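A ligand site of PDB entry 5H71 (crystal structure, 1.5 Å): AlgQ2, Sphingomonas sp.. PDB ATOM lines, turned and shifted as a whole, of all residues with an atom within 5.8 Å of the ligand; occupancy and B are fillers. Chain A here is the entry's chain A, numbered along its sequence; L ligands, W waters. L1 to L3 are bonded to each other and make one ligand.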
ATOM      1  N   ARG A  20     -14.255  11.103  31.541  1.00  0.00           N
ATOM      2  CA  ARG A  20     -14.702  12.349  30.925  1.00  0.00           C
ATOM      3  C   ARG A  20     -16.163  12.240  30.434  1.00  0.00           C
ATOM      4  O   ARG A  20     -16.579  12.907  29.474  1.00  0.00           O
ATOM      5  CB  ARG A  20     -13.703  12.738  29.809  1.00  0.00           C
ATOM      6  CG  ARG A  20     -12.324  13.133  30.419  1.00  0.00           C
ATOM      7  CD  ARG A  20     -11.059  13.143  29.508  1.00  0.00           C
ATOM      8  NE  ARG A  20      -9.851  13.407  30.302  1.00  0.00           N
ATOM      9  CZ  ARG A  20      -8.594  13.319  29.855  1.00  0.00           C
ATOM     10  NH1 ARG A  20      -8.352  12.967  28.604  1.00  0.00           N
ATOM     11  NH2 ARG A  20      -7.561  13.590  30.675  1.00  0.00           N
ATOM     12  N   LYS A  22     -17.753  10.193  28.756  1.00  0.00           N
ATOM     13  CA  LYS A  22     -17.998   9.849  27.352  1.00  0.00           C
ATOM     14  C   LYS A  22     -17.248   8.620  26.852  1.00  0.00           C
ATOM     15  O   LYS A  22     -17.666   7.997  25.876  1.00  0.00           O
ATOM     16  CB  LYS A  22     -17.596  11.016  26.448  1.00  0.00           C
ATOM     17  CG  LYS A  22     -18.499  12.246  26.507  1.00  0.00           C
ATOM     18  CD  LYS A  22     -17.988  13.306  25.530  1.00  0.00           C
ATOM     19  CE  LYS A  22     -16.588  13.824  25.917  1.00  0.00           C
ATOM     20  NZ  LYS A  22     -16.578  14.604  27.198  1.00  0.00           N
ATOM     21  N   ASP A  74     -10.792   9.159  35.559  1.00  0.00           N
ATOM     22  CA  ASP A  74     -10.518  10.486  36.093  1.00  0.00           C
ATOM     23  C   ASP A  74     -11.334  10.788  37.345  1.00  0.00           C
ATOM     24  O   ASP A  74     -12.422  10.229  37.554  1.00  0.00           O
ATOM     25  CB  ASP A  74     -10.760  11.552  35.017  1.00  0.00           C
ATOM     26  CG  ASP A  74     -12.161  11.499  34.413  1.00  0.00           C
ATOM     27  OD1 ASP A  74     -12.819  10.444  34.441  1.00  0.00           O
ATOM     28  OD2 ASP A  74     -12.590  12.548  33.871  1.00  0.00           O
ATOM     29  N   ASN A  75     -10.767  11.631  38.204  1.00  0.00           N
ATOM     30  CA  ASN A  75     -11.427  12.093  39.425  1.00  0.00           C
ATOM     31  C   ASN A  75     -11.848  10.960  40.338  1.00  0.00           C
ATOM     32  O   ASN A  75     -12.919  10.992  40.943  1.00  0.00           O
ATOM     33  CB  ASN A  75     -12.633  12.966  39.065  1.00  0.00           C
ATOM     34  CG  ASN A  75     -12.228  14.177  38.277  1.00  0.00           C
ATOM     35  OD1 ASN A  75     -11.340  14.919  38.703  1.00  0.00           O
ATOM     36  ND2 ASN A  75     -12.861  14.385  37.141  1.00  0.00           N
ATOM     37  N   TYR A 129      -2.105   9.344  37.247  1.00  0.00           N
ATOM     38  CA  TYR A 129      -1.715  10.170  36.106  1.00  0.00           C
ATOM     39  C   TYR A 129      -0.837  11.285  36.626  1.00  0.00           C
ATOM     40  O   TYR A 129      -1.297  12.141  37.384  1.00  0.00           O
ATOM     41  CB  TYR A 129      -2.994  10.692  35.411  1.00  0.00           C
ATOM     42  CG  TYR A 129      -2.849  11.821  34.418  1.00  0.00           C
ATOM     43  CD1 TYR A 129      -1.647  12.096  33.755  1.00  0.00           C
ATOM     44  CD2 TYR A 129      -3.962  12.604  34.107  1.00  0.00           C
ATOM     45  CE1 TYR A 129      -1.555  13.147  32.848  1.00  0.00           C
ATOM     46  CE2 TYR A 129      -3.876  13.634  33.178  1.00  0.00           C
ATOM     47  CZ  TYR A 129      -2.673  13.901  32.560  1.00  0.00           C
ATOM     48  OH  TYR A 129      -2.616  14.938  31.651  1.00  0.00           O
ATOM     49  N   ARG A 137      -3.937  26.662  32.034  1.00  0.00           N
ATOM     50  CA  ARG A 137      -4.703  27.613  31.225  1.00  0.00           C
ATOM     51  C   ARG A 137      -4.153  29.040  31.263  1.00  0.00           C
ATOM     52  O   ARG A 137      -3.361  29.406  32.148  1.00  0.00           O
ATOM     53  CB  ARG A 137      -6.160  27.621  31.688  1.00  0.00           C
ATOM     54  CG  ARG A 137      -6.905  26.331  31.393  1.00  0.00           C
ATOM     55  CD  ARG A 137      -8.255  26.292  32.100  1.00  0.00           C
ATOM     56  NE  ARG A 137      -8.993  25.081  31.777  1.00  0.00           N
ATOM     57  CZ  ARG A 137      -8.841  23.899  32.386  1.00  0.00           C
ATOM     58  NH1 ARG A 137      -7.976  23.750  33.370  1.00  0.00           N
ATOM     59  NH2 ARG A 137      -9.592  22.862  31.994  1.00  0.00           N
ATOM     60  N   ARG A 186     -14.914  25.578  26.606  1.00  0.00           N
ATOM     61  CA  ARG A 186     -15.289  24.163  26.551  1.00  0.00           C
ATOM     62  C   ARG A 186     -15.458  23.552  27.951  1.00  0.00           C
ATOM     63  O   ARG A 186     -16.028  22.470  28.072  1.00  0.00           O
ATOM     64  CB  ARG A 186     -14.264  23.368  25.743  1.00  0.00           C
ATOM     65  CG  ARG A 186     -12.830  23.553  26.204  1.00  0.00           C
ATOM     66  CD  ARG A 186     -11.969  22.413  25.717  1.00  0.00           C
ATOM     67  NE  ARG A 186     -10.551  22.657  25.958  1.00  0.00           N
ATOM     68  CZ  ARG A 186      -9.646  21.700  26.129  1.00  0.00           C
ATOM     69  NH1 ARG A 186      -9.999  20.415  26.112  1.00  0.00           N
ATOM     70  NH2 ARG A 186      -8.383  22.028  26.331  1.00  0.00           N
ATOM     71  N   HIS A 187     -14.960  24.210  28.989  1.00  0.00           N
ATOM     72  CA  HIS A 187     -15.195  23.766  30.365  1.00  0.00           C
ATOM     73  C   HIS A 187     -16.180  24.702  31.042  1.00  0.00           C
ATOM     74  O   HIS A 187     -15.853  25.868  31.323  1.00  0.00           O
ATOM     75  CB  HIS A 187     -13.886  23.680  31.142  1.00  0.00           C
ATOM     76  CG  HIS A 187     -12.978  22.612  30.633  1.00  0.00           C
ATOM     77  ND1 HIS A 187     -11.923  22.863  29.784  1.00  0.00           N
ATOM     78  CD2 HIS A 187     -12.983  21.278  30.838  1.00  0.00           C
ATOM     79  CE1 HIS A 187     -11.331  21.734  29.468  1.00  0.00           C
ATOM     80  NE2 HIS A 187     -11.946  20.748  30.103  1.00  0.00           N
ATOM     81  N   ASP A 206      -6.038  23.410  39.886  1.00  0.00           N
ATOM     82  CA  ASP A 206      -6.501  22.982  38.566  1.00  0.00           C
ATOM     83  C   ASP A 206      -7.706  22.035  38.631  1.00  0.00           C
ATOM     84  O   ASP A 206      -8.324  21.751  37.612  1.00  0.00           O
ATOM     85  CB  ASP A 206      -5.321  22.309  37.839  1.00  0.00           C
ATOM     86  CG  ASP A 206      -5.667  21.813  36.444  1.00  0.00           C
ATOM     87  OD1 ASP A 206      -6.003  22.639  35.552  1.00  0.00           O
ATOM     88  OD2 ASP A 206      -5.510  20.597  36.224  1.00  0.00           O
ATOM     89  N   ARG A 255     -14.624  25.070  21.206  1.00  0.00           N
ATOM     90  CA  ARG A 255     -13.695  25.851  20.386  1.00  0.00           C
ATOM     91  C   ARG A 255     -13.949  25.589  18.914  1.00  0.00           C
ATOM     92  O   ARG A 255     -13.987  26.516  18.099  1.00  0.00           O
ATOM     93  CB  ARG A 255     -12.248  25.530  20.758  1.00  0.00           C
ATOM     94  CG  ARG A 255     -11.939  25.932  22.193  1.00  0.00           C
ATOM     95  CD  ARG A 255     -10.523  25.567  22.589  1.00  0.00           C
ATOM     96  NE  ARG A 255     -10.335  24.114  22.571  1.00  0.00           N
ATOM     97  CZ  ARG A 255      -9.223  23.508  22.970  1.00  0.00           C
ATOM     98  NH1 ARG A 255      -8.209  24.233  23.427  1.00  0.00           N
ATOM     99  NH2 ARG A 255      -9.126  22.185  22.890  1.00  0.00           N
ATOM    100  N   ASP A 269      -8.280  28.850  28.533  1.00  0.00           N
ATOM    101  CA  ASP A 269      -8.074  27.474  28.122  1.00  0.00           C
ATOM    102  C   ASP A 269      -6.574  27.241  27.996  1.00  0.00           C
ATOM    103  O   ASP A 269      -5.777  28.160  28.224  1.00  0.00           O
ATOM    104  CB  ASP A 269      -8.819  27.209  26.789  1.00  0.00           C
ATOM    105  CG  ASP A 269      -9.123  25.722  26.532  1.00  0.00           C
ATOM    106  OD1 ASP A 269      -8.333  24.826  26.899  1.00  0.00           O
ATOM    107  OD2 ASP A 269     -10.171  25.470  25.888  1.00  0.00           O
ATOM    108  N   TRP A 270      -6.193  26.014  27.661  1.00  0.00           N
ATOM    109  CA  TRP A 270      -4.795  25.601  27.687  1.00  0.00           C
ATOM    110  C   TRP A 270      -4.016  26.232  26.552  1.00  0.00           C
ATOM    111  O   TRP A 270      -4.529  26.394  25.448  1.00  0.00           O
ATOM    112  CB  TRP A 270      -4.719  24.078  27.588  1.00  0.00           C
ATOM    113  CG  TRP A 270      -5.266  23.349  28.806  1.00  0.00           C
ATOM    114  CD1 TRP A 270      -6.587  23.234  29.175  1.00  0.00           C
ATOM    115  CD2 TRP A 270      -4.506  22.650  29.801  1.00  0.00           C
ATOM    116  NE1 TRP A 270      -6.689  22.521  30.343  1.00  0.00           N
ATOM    117  CE2 TRP A 270      -5.440  22.130  30.730  1.00  0.00           C
ATOM    118  CE3 TRP A 270      -3.141  22.393  29.980  1.00  0.00           C
ATOM    119  CZ2 TRP A 270      -5.042  21.389  31.854  1.00  0.00           C
ATOM    120  CZ3 TRP A 270      -2.747  21.642  31.082  1.00  0.00           C
ATOM    121  CH2 TRP A 270      -3.696  21.156  32.012  1.00  0.00           C
ATOM    122  N   PHE A 271      -2.758  26.582  26.804  1.00  0.00           N
ATOM    123  CA  PHE A 271      -1.954  27.251  25.783  1.00  0.00           C
ATOM    124  C   PHE A 271      -1.739  26.444  24.509  1.00  0.00           C
ATOM    125  O   PHE A 271      -1.937  26.978  23.413  1.00  0.00           O
ATOM    126  CB  PHE A 271      -0.593  27.630  26.377  1.00  0.00           C
ATOM    127  CG  PHE A 271      -0.629  28.858  27.252  1.00  0.00           C
ATOM    128  CD1 PHE A 271      -1.036  28.778  28.582  1.00  0.00           C
ATOM    129  CD2 PHE A 271      -0.222  30.088  26.755  1.00  0.00           C
ATOM    130  CE1 PHE A 271      -1.057  29.909  29.377  1.00  0.00           C
ATOM    131  CE2 PHE A 271      -0.246  31.230  27.537  1.00  0.00           C
ATOM    132  CZ  PHE A 271      -0.665  31.141  28.864  1.00  0.00           C
ATOM    133  N   ALA A 272      -1.338  25.173  24.621  1.00  0.00           N
ATOM    134  CA  ALA A 272      -0.951  24.463  23.405  1.00  0.00           C
ATOM    135  C   ALA A 272      -2.151  24.236  22.480  1.00  0.00           C
ATOM    136  O   ALA A 272      -2.107  24.634  21.324  1.00  0.00           O
ATOM    137  CB  ALA A 272      -0.258  23.157  23.726  1.00  0.00           C
ATOM    138  N   SER A 273      -3.229  23.632  22.981  1.00  0.00           N
ATOM    139  CA  SER A 273      -4.344  23.315  22.100  1.00  0.00           C
ATOM    140  C   SER A 273      -5.097  24.559  21.632  1.00  0.00           C
ATOM    141  O   SER A 273      -5.566  24.598  20.495  1.00  0.00           O
ATOM    142  CB  SER A 273      -5.315  22.345  22.773  1.00  0.00           C
ATOM    143  OG  SER A 273      -5.866  22.905  23.940  1.00  0.00           O
ATOM    144  N   THR A 274      -5.230  25.583  22.481  1.00  0.00           N
ATOM    145  CA  THR A 274      -6.008  26.752  22.087  1.00  0.00           C
ATOM    146  C   THR A 274      -5.270  27.484  20.968  1.00  0.00           C
ATOM    147  O   THR A 274      -5.882  27.947  20.006  1.00  0.00           O
ATOM    148  CB  THR A 274      -6.278  27.692  23.270  1.00  0.00           C
ATOM    149  OG1 THR A 274      -6.891  26.942  24.323  1.00  0.00           O
ATOM    150  CG2 THR A 274      -7.192  28.829  22.869  1.00  0.00           C
ATOM    151  N   ARG A 309      -0.469  23.660  36.316  1.00  0.00           N
ATOM    152  CA  ARG A 309      -0.337  22.244  36.086  1.00  0.00           C
ATOM    153  C   ARG A 309      -0.147  21.534  37.426  1.00  0.00           C
ATOM    154  O   ARG A 309       0.666  21.955  38.260  1.00  0.00           O
ATOM    155  CB  ARG A 309       0.820  21.948  35.102  1.00  0.00           C
ATOM    156  CG  ARG A 309       0.663  20.581  34.403  1.00  0.00           C
ATOM    157  CD  ARG A 309       0.183  20.665  32.952  1.00  0.00           C
ATOM    158  NE  ARG A 309       0.964  21.675  32.252  1.00  0.00           N
ATOM    159  CZ  ARG A 309       1.037  21.858  30.926  1.00  0.00           C
ATOM    160  NH1 ARG A 309       0.353  21.103  30.096  1.00  0.00           N
ATOM    161  NH2 ARG A 309       1.792  22.829  30.448  1.00  0.00           N
ATOM    162  N   ARG A 313      -2.420  14.282  39.115  1.00  0.00           N
ATOM    163  CA  ARG A 313      -3.863  14.476  38.987  1.00  0.00           C
ATOM    164  C   ARG A 313      -4.602  13.398  39.788  1.00  0.00           C
ATOM    165  O   ARG A 313      -4.022  12.340  40.078  1.00  0.00           O
ATOM    166  CB  ARG A 313      -4.302  14.468  37.498  1.00  0.00           C
ATOM    167  CG  ARG A 313      -4.418  15.899  36.898  1.00  0.00           C
ATOM    168  CD  ARG A 313      -5.307  15.963  35.642  1.00  0.00           C
ATOM    169  NE  ARG A 313      -6.609  15.382  35.952  1.00  0.00           N
ATOM    170  CZ  ARG A 313      -7.663  16.050  36.383  1.00  0.00           C
ATOM    171  NH1 ARG A 313      -7.644  17.379  36.477  1.00  0.00           N
ATOM    172  NH2 ARG A 313      -8.769  15.376  36.707  1.00  0.00           N
ATOM    173  N   ASP A 315      -6.425  11.092  39.152  1.00  0.00           N
ATOM    174  CA  ASP A 315      -6.830  10.108  38.157  1.00  0.00           C
ATOM    175  C   ASP A 315      -5.854   8.957  38.173  1.00  0.00           C
ATOM    176  O   ASP A 315      -4.705   9.141  38.574  1.00  0.00           O
ATOM    177  CB  ASP A 315      -6.817  10.669  36.710  1.00  0.00           C
ATOM    178  CG  ASP A 315      -7.409  12.071  36.561  1.00  0.00           C
ATOM    179  OD1 ASP A 315      -8.243  12.539  37.363  1.00  0.00           O
ATOM    180  OD2 ASP A 315      -7.018  12.716  35.539  1.00  0.00           O
ATOM    181  N   ASN A 375      -3.260  16.510  21.244  1.00  0.00           N
ATOM    182  CA  ASN A 375      -3.788  15.681  22.319  1.00  0.00           C
ATOM    183  C   ASN A 375      -5.140  15.061  21.952  1.00  0.00           C
ATOM    184  O   ASN A 375      -5.396  13.918  22.293  1.00  0.00           O
ATOM    185  CB  ASN A 375      -3.835  16.425  23.690  1.00  0.00           C
ATOM    186  CG  ASN A 375      -4.563  17.768  23.676  1.00  0.00           C
ATOM    187  OD1 ASN A 375      -5.009  18.275  22.657  1.00  0.00           O
ATOM    188  ND2 ASN A 375      -4.699  18.342  24.889  1.00  0.00           N
ATOM    189  N   TYR A 379      -6.048  11.126  22.078  1.00  0.00           N
ATOM    190  CA  TYR A 379      -7.211  10.556  22.768  1.00  0.00           C
ATOM    191  C   TYR A 379      -7.915   9.537  21.885  1.00  0.00           C
ATOM    192  O   TYR A 379      -8.371   8.492  22.351  1.00  0.00           O
ATOM    193  CB  TYR A 379      -8.233  11.625  23.155  1.00  0.00           C
ATOM    194  CG  TYR A 379      -7.789  12.752  24.052  1.00  0.00           C
ATOM    195  CD1 TYR A 379      -6.747  12.614  24.966  1.00  0.00           C
ATOM    196  CD2 TYR A 379      -8.417  13.989  23.960  1.00  0.00           C
ATOM    197  CE1 TYR A 379      -6.363  13.680  25.791  1.00  0.00           C
ATOM    198  CE2 TYR A 379      -8.053  15.049  24.778  1.00  0.00           C
ATOM    199  CZ  TYR A 379      -7.025  14.893  25.689  1.00  0.00           C
ATOM    200  OH  TYR A 379      -6.673  15.965  26.489  1.00  0.00           O
ATOM    201  N   GLN A 384      -2.614   9.727  25.957  1.00  0.00           N
ATOM    202  CA  GLN A 384      -2.945  10.895  26.796  1.00  0.00           C
ATOM    203  C   GLN A 384      -4.298  10.714  27.495  1.00  0.00           C
ATOM    204  O   GLN A 384      -5.096  11.658  27.662  1.00  0.00           O
ATOM    205  CB  GLN A 384      -2.943  12.202  25.964  1.00  0.00           C
ATOM    206  CG  GLN A 384      -1.591  12.560  25.352  1.00  0.00           C
ATOM    207  CD  GLN A 384      -0.500  12.825  26.392  1.00  0.00           C
ATOM    208  OE1 GLN A 384      -0.779  13.152  27.565  1.00  0.00           O
ATOM    209  NE2 GLN A 384       0.751  12.698  25.968  1.00  0.00           N
ATOM    210  N   GLN A 391       3.343  11.382  32.274  1.00  0.00           N
ATOM    211  CA  GLN A 391       3.321  12.245  31.104  1.00  0.00           C
ATOM    212  C   GLN A 391       4.723  12.806  30.836  1.00  0.00           C
ATOM    213  O   GLN A 391       5.537  12.953  31.745  1.00  0.00           O
ATOM    214  CB  GLN A 391       2.309  13.369  31.315  1.00  0.00           C
ATOM    215  CG  GLN A 391       1.945  14.087  30.023  1.00  0.00           C
ATOM    216  CD  GLN A 391       0.973  15.223  30.249  1.00  0.00           C
ATOM    217  OE1 GLN A 391       1.107  16.008  31.189  1.00  0.00           O
ATOM    218  NE2 GLN A 391      -0.037  15.324  29.373  1.00  0.00           N
ATOM    219  N   TYR A 395       6.296  15.694  24.591  1.00  0.00           N
ATOM    220  CA  TYR A 395       5.258  15.409  23.597  1.00  0.00           C
ATOM    221  C   TYR A 395       4.572  16.745  23.275  1.00  0.00           C
ATOM    222  O   TYR A 395       4.212  17.036  22.131  1.00  0.00           O
ATOM    223  CB  TYR A 395       4.214  14.367  24.042  1.00  0.00           C
ATOM    224  CG  TYR A 395       2.845  14.898  24.470  1.00  0.00           C
ATOM    225  CD1 TYR A 395       1.806  14.860  23.544  1.00  0.00           C
ATOM    226  CD2 TYR A 395       2.571  15.411  25.743  1.00  0.00           C
ATOM    227  CE1 TYR A 395       0.559  15.341  23.843  1.00  0.00           C
ATOM    228  CE2 TYR A 395       1.308  15.896  26.056  1.00  0.00           C
ATOM    229  CZ  TYR A 395       0.309  15.839  25.105  1.00  0.00           C
ATOM    230  OH  TYR A 395      -0.932  16.350  25.457  1.00  0.00           O
ATOM    231  N   GLU A 396       4.393  17.559  24.314  1.00  0.00           N
ATOM    232  CA  GLU A 396       3.628  18.795  24.232  1.00  0.00           C
ATOM    233  C   GLU A 396       4.446  19.912  23.600  1.00  0.00           C
ATOM    234  O   GLU A 396       3.932  20.728  22.833  1.00  0.00           O
ATOM    235  CB  GLU A 396       3.132  19.196  25.635  1.00  0.00           C
ATOM    236  CG  GLU A 396       2.199  20.378  25.611  1.00  0.00           C
ATOM    237  CD  GLU A 396       1.581  20.630  26.970  1.00  0.00           C
ATOM    238  OE1 GLU A 396       1.356  19.655  27.706  1.00  0.00           O
ATOM    239  OE2 GLU A 396       1.333  21.818  27.287  1.00  0.00           O
ATOM    240  N   TRP A 399       4.212  20.408  19.696  1.00  0.00           N
ATOM    241  CA  TRP A 399       3.098  21.079  19.050  1.00  0.00           C
ATOM    242  C   TRP A 399       2.690  22.344  19.804  1.00  0.00           C
ATOM    243  O   TRP A 399       1.596  22.860  19.606  1.00  0.00           O
ATOM    244  CB  TRP A 399       1.901  20.145  18.869  1.00  0.00           C
ATOM    245  CG  TRP A 399       1.415  19.434  20.109  1.00  0.00           C
ATOM    246  CD1 TRP A 399       1.987  18.355  20.691  1.00  0.00           C
ATOM    247  CD2 TRP A 399       0.244  19.737  20.870  1.00  0.00           C
ATOM    248  NE1 TRP A 399       1.264  17.968  21.810  1.00  0.00           N
ATOM    249  CE2 TRP A 399       0.186  18.796  21.931  1.00  0.00           C
ATOM    250  CE3 TRP A 399      -0.761  20.718  20.764  1.00  0.00           C
ATOM    251  CZ2 TRP A 399      -0.841  18.808  22.892  1.00  0.00           C
ATOM    252  CZ3 TRP A 399      -1.787  20.719  21.716  1.00  0.00           C
ATOM    253  CH2 TRP A 399      -1.810  19.771  22.770  1.00  0.00           C
HETATM  254  C1  LIG L   1     -12.658  16.631  34.082  1.00  0.00           C
HETATM  255  C2  LIG L   1     -11.239  16.096  34.261  1.00  0.00           C
HETATM  256  O1  LIG L   1     -11.073  14.806  33.672  1.00  0.00           O
HETATM  257  C3  LIG L   1     -10.310  17.001  33.502  1.00  0.00           C
HETATM  258  O2  LIG L   1      -8.995  16.466  33.639  1.00  0.00           O
HETATM  259  C4  LIG L   1     -10.705  17.086  32.031  1.00  0.00           C
HETATM  260  O3  LIG L   1     -10.057  18.243  31.532  1.00  0.00           O
HETATM  261  C5  LIG L   1     -12.178  17.429  31.863  1.00  0.00           C
HETATM  262  O4  LIG L   1     -12.964  16.567  32.696  1.00  0.00           O
HETATM  263  C6  LIG L   1     -12.566  17.197  30.432  1.00  0.00           C
HETATM  264  O5  LIG L   1     -12.183  18.011  29.561  1.00  0.00           O
HETATM  265  O6  LIG L   1     -13.255  16.201  30.148  1.00  0.00           O
HETATM  266  O7  LIG L   1     -13.591  15.870  34.843  1.00  0.00           O
HETATM  267  C1  LG2 L   2      -8.995  17.878  30.658  1.00  0.00           C
HETATM  268  C2  LG2 L   2      -8.727  19.096  29.781  1.00  0.00           C
HETATM  269  O1  LG2 L   2      -8.509  20.238  30.617  1.00  0.00           O
HETATM  270  C3  LG2 L   2      -7.508  18.852  28.935  1.00  0.00           C
HETATM  271  O2  LG2 L   2      -7.178  20.050  28.215  1.00  0.00           O
HETATM  272  C4  LG2 L   2      -6.321  18.426  29.788  1.00  0.00           C
HETATM  273  O3  LG2 L   2      -5.290  17.925  28.950  1.00  0.00           O
HETATM  274  C5  LG2 L   2      -6.742  17.219  30.613  1.00  0.00           C
HETATM  275  O4  LG2 L   2      -7.818  17.605  31.425  1.00  0.00           O
HETATM  276  C6  LG2 L   2      -5.568  16.826  31.458  1.00  0.00           C
HETATM  277  O5  LG2 L   2      -5.346  17.401  32.533  1.00  0.00           O
HETATM  278  O6  LG2 L   2      -4.807  15.954  30.997  1.00  0.00           O
HETATM  279  C1  LG3 L   3      -4.186  18.819  28.784  1.00  0.00           C
HETATM  280  C2  LG3 L   3      -2.979  17.957  28.448  1.00  0.00           C
HETATM  281  O1  LG3 L   3      -3.305  17.126  27.316  1.00  0.00           O
HETATM  282  C3  LG3 L   3      -1.775  18.846  28.150  1.00  0.00           C
HETATM  283  O2  LG3 L   3      -0.737  17.986  27.669  1.00  0.00           O
HETATM  284  C4  LG3 L   3      -2.149  19.912  27.150  1.00  0.00           C
HETATM  285  C5  LG3 L   3      -3.430  20.275  26.982  1.00  0.00           C
HETATM  286  O3  LG3 L   3      -4.510  19.678  27.698  1.00  0.00           O
HETATM  287  C6  LG3 L   3      -3.870  21.275  26.028  1.00  0.00           C
HETATM  288  O4  LG3 L   3      -3.059  22.080  25.548  1.00  0.00           O
HETATM  289  O5  LG3 L   3      -5.097  21.233  25.721  1.00  0.00           O
HETATM  290  O   HOH W   1     -13.758  18.495  27.394  1.00  0.00           O
HETATM  291  O   HOH W   2      -8.109  18.386  25.513  1.00  0.00           O
HETATM  292  O   HOH W   3      -8.376  13.727  33.399  1.00  0.00           O
HETATM  293  O   HOH W   4     -15.622  15.576  31.714  1.00  0.00           O
HETATM  294  O   HOH W   5     -13.982  15.827  27.218  1.00  0.00           O
HETATM  295  O   HOH W   6      -4.909  15.076  28.410  1.00  0.00           O
HETATM  296  O   HOH W   7      -2.848  17.621  33.626  1.00  0.00           O
HETATM  297  O   HOH W   8      -8.932  20.596  33.616  1.00  0.00           O
HETATM  298  O   HOH W   9     -16.073  14.669  33.891  1.00  0.00           O
HETATM  299  O   HOH W  10      -1.034  23.309  26.909  1.00  0.00           O
HETATM  300  O   HOH W  11      -6.651  19.089  34.243  1.00  0.00           O
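The side-chain hydroxyl of Tyr 129 sits at hydrogen-bond distance from an oxygen (O6) of LG2 L2 (2.5 Å). The backbone NH (N) of Ser 273 lies within hydrogen-bond range of an oxygen (O4) of LG3 L3 (3.0 Å). OG of Ser 273 sits at hydrogen-bond distance from O5 of LG3 L3 (2.6 Å). The side-chain carboxylate (OE1) of Glu 396 lies within hydrogen-bond range of an oxygen (O2) of LG3 L3 (2.7 Å). OD2 of Asp 74 sits at hydrogen-bond distance from O1 of LIG L1 (2.7 Å). An oxygen (O2) of LG3 L3 lies within hydrogen-bond range of the side-chain hydroxyl (OH) of Tyr 395. A ring nitrogen (NE2) of His 187 sits at hydrogen-bond distance from an oxygen (O5) of LIG L1, at 2.8 Å. The side-chain amide nitrogen of Asn 75 is in hydrogen-bond range of an oxygen (O7) of LIG L1 (2.8 Å). NE1 of Trp 270 is in hydrogen-bond range of O1 of LG2 L2 (2.9 Å). NH2 of Arg 186 lies within salt-bridge range of O5 of LG3 L3 (3.4 Å). An oxygen (O5) of LG3 L3 lies within hydrogen-bond range of the side-chain amide nitrogen of Asn 375 (3.0 Å). An oxygen (O2) of LIG L1 sits close to the guanidinium group (NH2) of Arg 313, at 3.3 Å. O1 of LG2 L2 is in hydrogen-bond range of NH2 of Arg 137 (3.2 Å). An oxygen (O6) of LG2 L2 lies within salt-bridge range of the guanidinium group (NH2) of Arg 20. O2 of LG3 L3 lies within hydrogen-bond range of NE2 of Gln 391 (3.2 Å). The side-chain hydroxyl (OH) of Tyr 379 sits at hydrogen-bond distance from an oxygen (O3) of LG2 L2.
The backbone carbonyl oxygen of Tyr 129 sits at hydrogen-bond distance from the backbone NH of Arg 313 (3.0 Å). OE1 of Glu 396 is in salt-bridge range of NH1 of Arg 309, 3.0 Å away. O of Tyr 395 sits close to NE1 of Trp 399 (3.1 Å). N of Asn 75 lies within hydrogen-bond range of OD1 of Asp 315, at 2.8 Å. The side-chain hydroxyl of Thr 274 is in hydrogen-bond range of the backbone carbonyl oxygen of Trp 270 (2.7 Å). The guanidinium group (NE) of Arg 313 is in salt-bridge range of the side-chain carboxylate (OD2) of Asp 315, at 2.7 Å. The guanidinium group (NH1) of Arg 137 lies within salt-bridge range of the side-chain carboxylate (OD1) of Asp 206, at 3.1 Å. NZ of Lys 22 lies within hydrogen-bond range of O of Arg 20 (2.8 Å).
CB of Ala 272 touches O4 of LG3 L3, at 3.5 Å. Arg 309 touches the ligand. CH2 of Trp 399 touches O4 of LG3 L3, 3.8 Å away. Hydrophobic or aromatic side chains within 4 Å of the ligand: Tyr 129, His 187, Trp 270, Ala 272, Tyr 395 and Trp 399. The nearest printed residue that does not touch the ligand is Asp 315 (4.6 Å).
Water W10 lies within hydrogen-bond range of an oxygen (O4) of LG3 L3 (2.7 Å), the side-chain carboxylate of Glu 396 (2.8 Å) and the backbone NH of Ala 272 (3.0 Å). Water W6 bridges O6 of LG2 L2 (2.7 Å) and OH of Tyr 379 (2.8 Å). Water W11 lies within hydrogen-bond range of O5 of LG2 L2, OD2 of Asp 206 and NH1 of Arg 313. Water W7 bridges O5 of LG2 L2 (2.7 Å) and OH of Tyr 129 (3.3 Å). Water W3 lies within hydrogen-bond range of OD2 of Asp 315, O2 of LIG L1 and NH2 of Arg 20. Water W2 lies within hydrogen-bond range of the guanidinium group of Arg 186, the side-chain hydroxyl of Tyr 379, an oxygen (O2) of LG2 L2 and the side-chain amide nitrogen of Asn 375.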
